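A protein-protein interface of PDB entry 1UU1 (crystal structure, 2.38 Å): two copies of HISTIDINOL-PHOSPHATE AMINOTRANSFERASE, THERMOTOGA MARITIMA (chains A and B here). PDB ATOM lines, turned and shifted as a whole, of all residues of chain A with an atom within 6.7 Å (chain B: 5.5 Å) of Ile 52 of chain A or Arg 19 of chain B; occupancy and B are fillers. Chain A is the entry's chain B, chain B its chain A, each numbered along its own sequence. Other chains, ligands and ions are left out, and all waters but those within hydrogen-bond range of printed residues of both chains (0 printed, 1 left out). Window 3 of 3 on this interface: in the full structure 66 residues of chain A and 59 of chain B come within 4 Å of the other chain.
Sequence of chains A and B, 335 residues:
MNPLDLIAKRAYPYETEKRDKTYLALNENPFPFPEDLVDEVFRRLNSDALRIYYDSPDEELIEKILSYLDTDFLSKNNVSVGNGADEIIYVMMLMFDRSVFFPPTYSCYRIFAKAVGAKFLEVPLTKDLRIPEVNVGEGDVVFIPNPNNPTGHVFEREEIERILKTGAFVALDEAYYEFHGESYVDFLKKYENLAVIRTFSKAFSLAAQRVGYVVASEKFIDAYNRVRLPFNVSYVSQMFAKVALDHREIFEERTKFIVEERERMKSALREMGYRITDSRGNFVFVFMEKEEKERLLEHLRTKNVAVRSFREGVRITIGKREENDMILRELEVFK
Among the printed residues, merely in contact across the chains: Ala 49 of chain A with Ala 208 of chain B (3.3 Å), Ile 52 of chain A with Glu 28 of chain B (3.4 Å), Arg 51 of chain A with Glu 28 of chain B (3.4 Å), Ile 52 of chain A with Ala 207 of chain B (3.5 Å), Arg 51 of chain A with Ala 207 of chain B (3.6 Å), Tyr 53 of chain A with Arg 19 of chain B (3.6 Å), Tyr 53 of chain A with Leu 26 of chain B (3.7 Å), Ile 52 of chain A with Arg 19 of chain B (3.7 Å), Asp 55 of chain A with Thr 16 of chain B (3.7 Å) and Tyr 53 of chain A with Ala 207 of chain B (3.8 Å).
The backbone NH (N) of Tyr 53 of chain A lies within hydrogen-bond range of the side-chain carboxylate (OE1) of Glu 28 of chain B (3.0 Å).
The backbone NH (N) of Ala 207 of chain B sits at hydrogen-bond distance from the backbone carbonyl oxygen (O) of Leu 50 of chain A.
N of Ala 208 of chain B is in hydrogen-bond range of O of Leu 50 of chain A (3.0 Å).
The backbone NH of Ala 208 of chain B lies within hydrogen-bond range of the backbone carbonyl oxygen of Ile 52 of chain A, at 3.0 Å.
The backbone carbonyl oxygen (O) of Ala 208 of chain B sits at hydrogen-bond distance from the backbone NH (N) of Tyr 235 of chain A.
No position is printed for both chains.
Hydrophobic or aromatic side chains of chain A that line the printed part of chain B: Ile 52, Tyr 53 and Tyr 235.
Hydrophobic or aromatic side chains of chain B that line the printed part of chain A: Ala 207 and Ala 208.
Among the printed residues, no Asp or Glu carboxylate lies within 4 Å of a Lys or Arg side-chain nitrogen of the other chain.
The guanidinium group (NH2) of Arg 19 of chain B lies within salt-bridge range of the side-chain carboxylate (OE2) of Glu 28 of chain B, 2.6 Å away.
The guanidinium group of Arg 51 of chain A is in salt-bridge range of the side-chain carboxylate of Asp 48 of chain A, 3.3 Å away.
Of the printed residues of chain A, Arg 19 of chain B touches Ile 52 (3.7 Å) and Tyr 53 (3.6 Å).
Printed residues of chain B within 4 Å of Tyr 53 of chain A: Arg 19, Leu 26, Glu 28 and Ala 207.
Printed residues of chain B within 4 Å of Leu 50 of chain A: Ala 207 and Ala 208.
Of the printed residues of chain B, Arg 51 of chain A touches Glu 28 and Ala 207.
Glu 17 of chain B touches none of the printed residues of chain A.
Asp 20 of chain B touches none of the printed residues of chain A.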
ATOM      1  N   ASP A  48      15.712  19.705  15.009  1.00  0.00           N
ATOM      2  CA  ASP A  48      16.403  19.603  13.748  1.00  0.00           C
ATOM      3  C   ASP A  48      17.079  18.238  13.593  1.00  0.00           C
ATOM      4  O   ASP A  48      17.349  17.798  12.478  1.00  0.00           O
ATOM      5  CB  ASP A  48      17.445  20.712  13.622  1.00  0.00           C
ATOM      6  CG  ASP A  48      17.934  20.882  12.206  1.00  0.00           C
ATOM      7  OD1 ASP A  48      19.114  20.569  11.914  1.00  0.00           O
ATOM      8  OD2 ASP A  48      17.115  21.317  11.383  1.00  0.00           O
ATOM      9  N   ALA A  49      17.354  17.572  14.708  1.00  0.00           N
ATOM     10  CA  ALA A  49      17.998  16.266  14.681  1.00  0.00           C
ATOM     11  C   ALA A  49      17.016  15.183  14.205  1.00  0.00           C
ATOM     12  O   ALA A  49      17.436  14.093  13.766  1.00  0.00           O
ATOM     13  CB  ALA A  49      18.515  15.914  16.070  1.00  0.00           C
ATOM     14  N   LEU A  50      15.719  15.468  14.286  1.00  0.00           N
ATOM     15  CA  LEU A  50      14.715  14.493  13.860  1.00  0.00           C
ATOM     16  C   LEU A  50      14.733  14.170  12.355  1.00  0.00           C
ATOM     17  O   LEU A  50      14.370  13.063  11.961  1.00  0.00           O
ATOM     18  CB  LEU A  50      13.296  14.962  14.260  1.00  0.00           C
ATOM     19  CG  LEU A  50      12.989  14.899  15.757  1.00  0.00           C
ATOM     20  CD1 LEU A  50      11.625  15.494  16.040  1.00  0.00           C
ATOM     21  CD2 LEU A  50      13.065  13.462  16.246  1.00  0.00           C
ATOM     22  N   ARG A  51      15.128  15.148  11.541  1.00  0.00           N
ATOM     23  CA  ARG A  51      15.176  15.013  10.079  1.00  0.00           C
ATOM     24  C   ARG A  51      16.412  14.261   9.548  1.00  0.00           C
ATOM     25  O   ARG A  51      16.515  13.993   8.343  1.00  0.00           O
ATOM     26  CB  ARG A  51      15.199  16.400   9.418  1.00  0.00           C
ATOM     27  CG  ARG A  51      16.518  17.137   9.660  1.00  0.00           C
ATOM     28  CD  ARG A  51      16.561  18.510   9.020  1.00  0.00           C
ATOM     29  NE  ARG A  51      17.418  18.535   7.837  1.00  0.00           N
ATOM     30  CZ  ARG A  51      18.731  18.743   7.852  1.00  0.00           C
ATOM     31  NH1 ARG A  51      19.402  18.740   6.713  1.00  0.00           N
ATOM     32  NH2 ARG A  51      19.377  18.974   8.992  1.00  0.00           N
ATOM     33  N   ILE A  52      17.341  13.922  10.428  1.00  0.00           N
ATOM     34  CA  ILE A  52      18.548  13.286   9.935  1.00  0.00           C
ATOM     35  C   ILE A  52      18.630  11.846  10.347  1.00  0.00           C
ATOM     36  O   ILE A  52      17.885  11.399  11.201  1.00  0.00           O
ATOM     37  CB  ILE A  52      19.822  14.001  10.449  1.00  0.00           C
ATOM     38  CG1 ILE A  52      19.933  13.830  11.972  1.00  0.00           C
ATOM     39  CG2 ILE A  52      19.748  15.488  10.123  1.00  0.00           C
ATOM     40  CD1 ILE A  52      21.291  14.194  12.516  1.00  0.00           C
ATOM     41  N   TYR A  53      19.536  11.124   9.704  1.00  0.00           N
ATOM     42  CA  TYR A  53      19.763   9.741  10.016  1.00  0.00           C
ATOM     43  C   TYR A  53      20.697   9.868  11.197  1.00  0.00           C
ATOM     44  O   TYR A  53      21.762  10.479  11.086  1.00  0.00           O
ATOM     45  CB  TYR A  53      20.364   9.053   8.789  1.00  0.00           C
ATOM     46  CG  TYR A  53      19.263   8.679   7.816  1.00  0.00           C
ATOM     47  CD1 TYR A  53      18.498   7.520   8.010  1.00  0.00           C
ATOM     48  CD2 TYR A  53      18.922   9.526   6.752  1.00  0.00           C
ATOM     49  CE1 TYR A  53      17.411   7.217   7.168  1.00  0.00           C
ATOM     50  CE2 TYR A  53      17.842   9.235   5.905  1.00  0.00           C
ATOM     51  CZ  TYR A  53      17.090   8.083   6.117  1.00  0.00           C
ATOM     52  OH  TYR A  53      16.038   7.795   5.282  1.00  0.00           O
ATOM     53  N   TYR A  54      20.234   9.359  12.340  1.00  0.00           N
ATOM     54  CA  TYR A  54      20.961   9.477  13.592  1.00  0.00           C
ATOM     55  C   TYR A  54      21.729   8.207  13.989  1.00  0.00           C
ATOM     56  O   TYR A  54      21.155   7.133  14.136  1.00  0.00           O
ATOM     57  CB  TYR A  54      19.969   9.904  14.705  1.00  0.00           C
ATOM     58  CG  TYR A  54      20.613  10.536  15.929  1.00  0.00           C
ATOM     59  CD1 TYR A  54      21.009  11.877  15.935  1.00  0.00           C
ATOM     60  CD2 TYR A  54      20.904   9.771  17.049  1.00  0.00           C
ATOM     61  CE1 TYR A  54      21.702  12.422  17.028  1.00  0.00           C
ATOM     62  CE2 TYR A  54      21.583  10.309  18.137  1.00  0.00           C
ATOM     63  CZ  TYR A  54      21.987  11.615  18.112  1.00  0.00           C
ATOM     64  OH  TYR A  54      22.759  12.077  19.146  1.00  0.00           O
ATOM     65  N   ASP A  55      23.046   8.344  14.128  1.00  0.00           N
ATOM     66  CA  ASP A  55      23.933   7.243  14.505  1.00  0.00           C
ATOM     67  C   ASP A  55      23.229   6.452  15.567  1.00  0.00           C
ATOM     68  O   ASP A  55      22.925   6.973  16.633  1.00  0.00           O
ATOM     69  CB  ASP A  55      25.274   7.807  14.987  1.00  0.00           C
ATOM     70  CG  ASP A  55      26.052   8.494  13.844  1.00  0.00           C
ATOM     71  OD1 ASP A  55      27.156   9.041  14.036  1.00  0.00           O
ATOM     72  OD2 ASP A  55      25.531   8.475  12.707  1.00  0.00           O
ATOM     73  N   TYR A 235      16.649   8.219  17.553  1.00  0.00           N
ATOM     74  CA  TYR A 235      17.299   9.299  18.237  1.00  0.00           C
ATOM     75  C   TYR A 235      16.571   9.480  19.588  1.00  0.00           C
ATOM     76  O   TYR A 235      17.205   9.562  20.639  1.00  0.00           O
ATOM     77  CB  TYR A 235      17.196  10.552  17.360  1.00  0.00           C
ATOM     78  CG  TYR A 235      17.438  11.865  18.067  1.00  0.00           C
ATOM     79  CD1 TYR A 235      18.702  12.209  18.564  1.00  0.00           C
ATOM     80  CD2 TYR A 235      16.410  12.782  18.202  1.00  0.00           C
ATOM     81  CE1 TYR A 235      18.929  13.445  19.176  1.00  0.00           C
ATOM     82  CE2 TYR A 235      16.613  14.020  18.805  1.00  0.00           C
ATOM     83  CZ  TYR A 235      17.860  14.351  19.288  1.00  0.00           C
ATOM     84  OH  TYR A 235      18.016  15.588  19.864  1.00  0.00           O
ATOM     85  N   THR B  16      30.050   6.126  10.122  1.00  0.00           N
ATOM     86  CA  THR B  16      29.548   7.373   9.549  1.00  0.00           C
ATOM     87  C   THR B  16      30.522   8.516   9.820  1.00  0.00           C
ATOM     88  O   THR B  16      30.415   9.196  10.844  1.00  0.00           O
ATOM     89  CB  THR B  16      28.162   7.751  10.140  1.00  0.00           C
ATOM     90  OG1 THR B  16      27.190   6.768   9.759  1.00  0.00           O
ATOM     91  CG2 THR B  16      27.713   9.124   9.630  1.00  0.00           C
ATOM     92  N   GLU B  17      31.472   8.719   8.903  1.00  0.00           N
ATOM     93  CA  GLU B  17      32.461   9.792   9.043  1.00  0.00           C
ATOM     94  C   GLU B  17      31.769  11.099   9.406  1.00  0.00           C
ATOM     95  O   GLU B  17      30.570  11.262   9.166  1.00  0.00           O
ATOM     96  CB  GLU B  17      33.262   9.978   7.744  1.00  0.00           C
ATOM     97  CG  GLU B  17      34.597   9.232   7.697  1.00  0.00           C
ATOM     98  CD  GLU B  17      34.446   7.718   7.630  1.00  0.00           C
ATOM     99  OE1 GLU B  17      35.480   7.016   7.628  1.00  0.00           O
ATOM    100  OE2 GLU B  17      33.297   7.228   7.577  1.00  0.00           O
ATOM    101  N   LYS B  18      32.526  12.026   9.983  1.00  0.00           N
ATOM    102  CA  LYS B  18      31.973  13.314  10.391  1.00  0.00           C
ATOM    103  C   LYS B  18      31.263  14.044   9.256  1.00  0.00           C
ATOM    104  O   LYS B  18      31.886  14.463   8.280  1.00  0.00           O
ATOM    105  CB  LYS B  18      33.071  14.214  10.967  1.00  0.00           C
ATOM    106  CG  LYS B  18      32.777  14.675  12.379  1.00  0.00           C
ATOM    107  CD  LYS B  18      31.457  15.425  12.432  1.00  0.00           C
ATOM    108  CE  LYS B  18      30.716  15.145  13.730  1.00  0.00           C
ATOM    109  NZ  LYS B  18      29.409  15.860  13.789  1.00  0.00           N
ATOM    110  N   ARG B  19      29.951  14.192   9.396  1.00  0.00           N
ATOM    111  CA  ARG B  19      29.155  14.879   8.395  1.00  0.00           C
ATOM    112  C   ARG B  19      29.679  16.296   8.251  1.00  0.00           C
ATOM    113  O   ARG B  19      29.945  16.972   9.239  1.00  0.00           O
ATOM    114  CB  ARG B  19      27.693  14.927   8.831  1.00  0.00           C
ATOM    115  CG  ARG B  19      27.060  13.572   9.041  1.00  0.00           C
ATOM    116  CD  ARG B  19      25.786  13.713   9.848  1.00  0.00           C
ATOM    117  NE  ARG B  19      24.770  14.514   9.172  1.00  0.00           N
ATOM    118  CZ  ARG B  19      23.638  14.019   8.672  1.00  0.00           C
ATOM    119  NH1 ARG B  19      23.370  12.714   8.765  1.00  0.00           N
ATOM    120  NH2 ARG B  19      22.773  14.827   8.070  1.00  0.00           N
ATOM    121  N   ASP B  20      29.848  16.736   7.015  1.00  0.00           N
ATOM    122  CA  ASP B  20      30.310  18.080   6.754  1.00  0.00           C
ATOM    123  C   ASP B  20      29.215  19.029   7.204  1.00  0.00           C
ATOM    124  O   ASP B  20      28.066  18.625   7.387  1.00  0.00           O
ATOM    125  CB  ASP B  20      30.571  18.266   5.268  1.00  0.00           C
ATOM    126  CG  ASP B  20      32.028  18.174   4.924  1.00  0.00           C
ATOM    127  OD1 ASP B  20      32.805  18.925   5.539  1.00  0.00           O
ATOM    128  OD2 ASP B  20      32.393  17.366   4.042  1.00  0.00           O
ATOM    129  N   LYS B  21      29.575  20.296   7.361  1.00  0.00           N
ATOM    130  CA  LYS B  21      28.636  21.311   7.803  1.00  0.00           C
ATOM    131  C   LYS B  21      27.367  21.309   6.956  1.00  0.00           C
ATOM    132  O   LYS B  21      26.273  21.134   7.478  1.00  0.00           O
ATOM    133  CB  LYS B  21      29.299  22.689   7.772  1.00  0.00           C
ATOM    134  CG  LYS B  21      30.758  22.715   8.266  1.00  0.00           C
ATOM    135  CD  LYS B  21      31.013  21.846   9.516  1.00  0.00           C
ATOM    136  CE  LYS B  21      30.213  22.286  10.741  1.00  0.00           C
ATOM    137  NZ  LYS B  21      30.726  21.627  11.980  1.00  0.00           N
ATOM    138  N   TYR B  23      25.402  19.257   4.789  1.00  0.00           N
ATOM    139  CA  TYR B  23      25.219  17.861   4.424  1.00  0.00           C
ATOM    140  C   TYR B  23      24.057  17.660   3.447  1.00  0.00           C
ATOM    141  O   TYR B  23      22.899  17.814   3.820  1.00  0.00           O
ATOM    142  CB  TYR B  23      24.957  17.054   5.704  1.00  0.00           C
ATOM    143  CG  TYR B  23      25.284  15.587   5.599  1.00  0.00           C
ATOM    144  CD1 TYR B  23      26.615  15.144   5.625  1.00  0.00           C
ATOM    145  CD2 TYR B  23      24.271  14.650   5.408  1.00  0.00           C
ATOM    146  CE1 TYR B  23      26.934  13.800   5.450  1.00  0.00           C
ATOM    147  CE2 TYR B  23      24.575  13.310   5.233  1.00  0.00           C
ATOM    148  CZ  TYR B  23      25.911  12.888   5.249  1.00  0.00           C
ATOM    149  OH  TYR B  23      26.215  11.558   5.024  1.00  0.00           O
ATOM    150  N   LEU B  26      22.318  12.445   2.156  1.00  0.00           N
ATOM    151  CA  LEU B  26      21.435  11.364   2.595  1.00  0.00           C
ATOM    152  C   LEU B  26      19.961  11.586   2.294  1.00  0.00           C
ATOM    153  O   LEU B  26      19.097  11.021   2.969  1.00  0.00           O
ATOM    154  CB  LEU B  26      21.603  11.094   4.097  1.00  0.00           C
ATOM    155  CG  LEU B  26      22.818  10.258   4.484  1.00  0.00           C
ATOM    156  CD1 LEU B  26      22.986  10.254   5.973  1.00  0.00           C
ATOM    157  CD2 LEU B  26      22.667   8.833   3.943  1.00  0.00           C
ATOM    158  N   GLU B  28      17.989  13.601   3.115  1.00  0.00           N
ATOM    159  CA  GLU B  28      17.274  14.025   4.310  1.00  0.00           C
ATOM    160  C   GLU B  28      16.421  15.313   4.033  1.00  0.00           C
ATOM    161  O   GLU B  28      16.811  16.205   3.257  1.00  0.00           O
ATOM    162  CB  GLU B  28      18.293  14.306   5.422  1.00  0.00           C
ATOM    163  CG  GLU B  28      19.055  13.078   5.931  1.00  0.00           C
ATOM    164  CD  GLU B  28      20.395  13.423   6.564  1.00  0.00           C
ATOM    165  OE1 GLU B  28      20.806  12.669   7.468  1.00  0.00           O
ATOM    166  OE2 GLU B  28      21.045  14.428   6.162  1.00  0.00           O
ATOM    167  N   ALA B 207      13.512  10.959   9.772  1.00  0.00           N
ATOM    168  CA  ALA B 207      14.514   9.942   9.505  1.00  0.00           C
ATOM    169  C   ALA B 207      15.096   9.318  10.767  1.00  0.00           C
ATOM    170  O   ALA B 207      15.366   8.112  10.812  1.00  0.00           O
ATOM    171  CB  ALA B 207      15.596  10.537   8.653  1.00  0.00           C
ATOM    172  N   ALA B 208      15.252  10.153  11.795  1.00  0.00           N
ATOM    173  CA  ALA B 208      15.796   9.760  13.079  1.00  0.00           C
ATOM    174  C   ALA B 208      14.913   8.854  13.928  1.00  0.00           C
ATOM    175  O   ALA B 208      15.443   8.191  14.801  1.00  0.00           O
ATOM    176  CB  ALA B 208      16.159  11.009  13.890  1.00  0.00           C
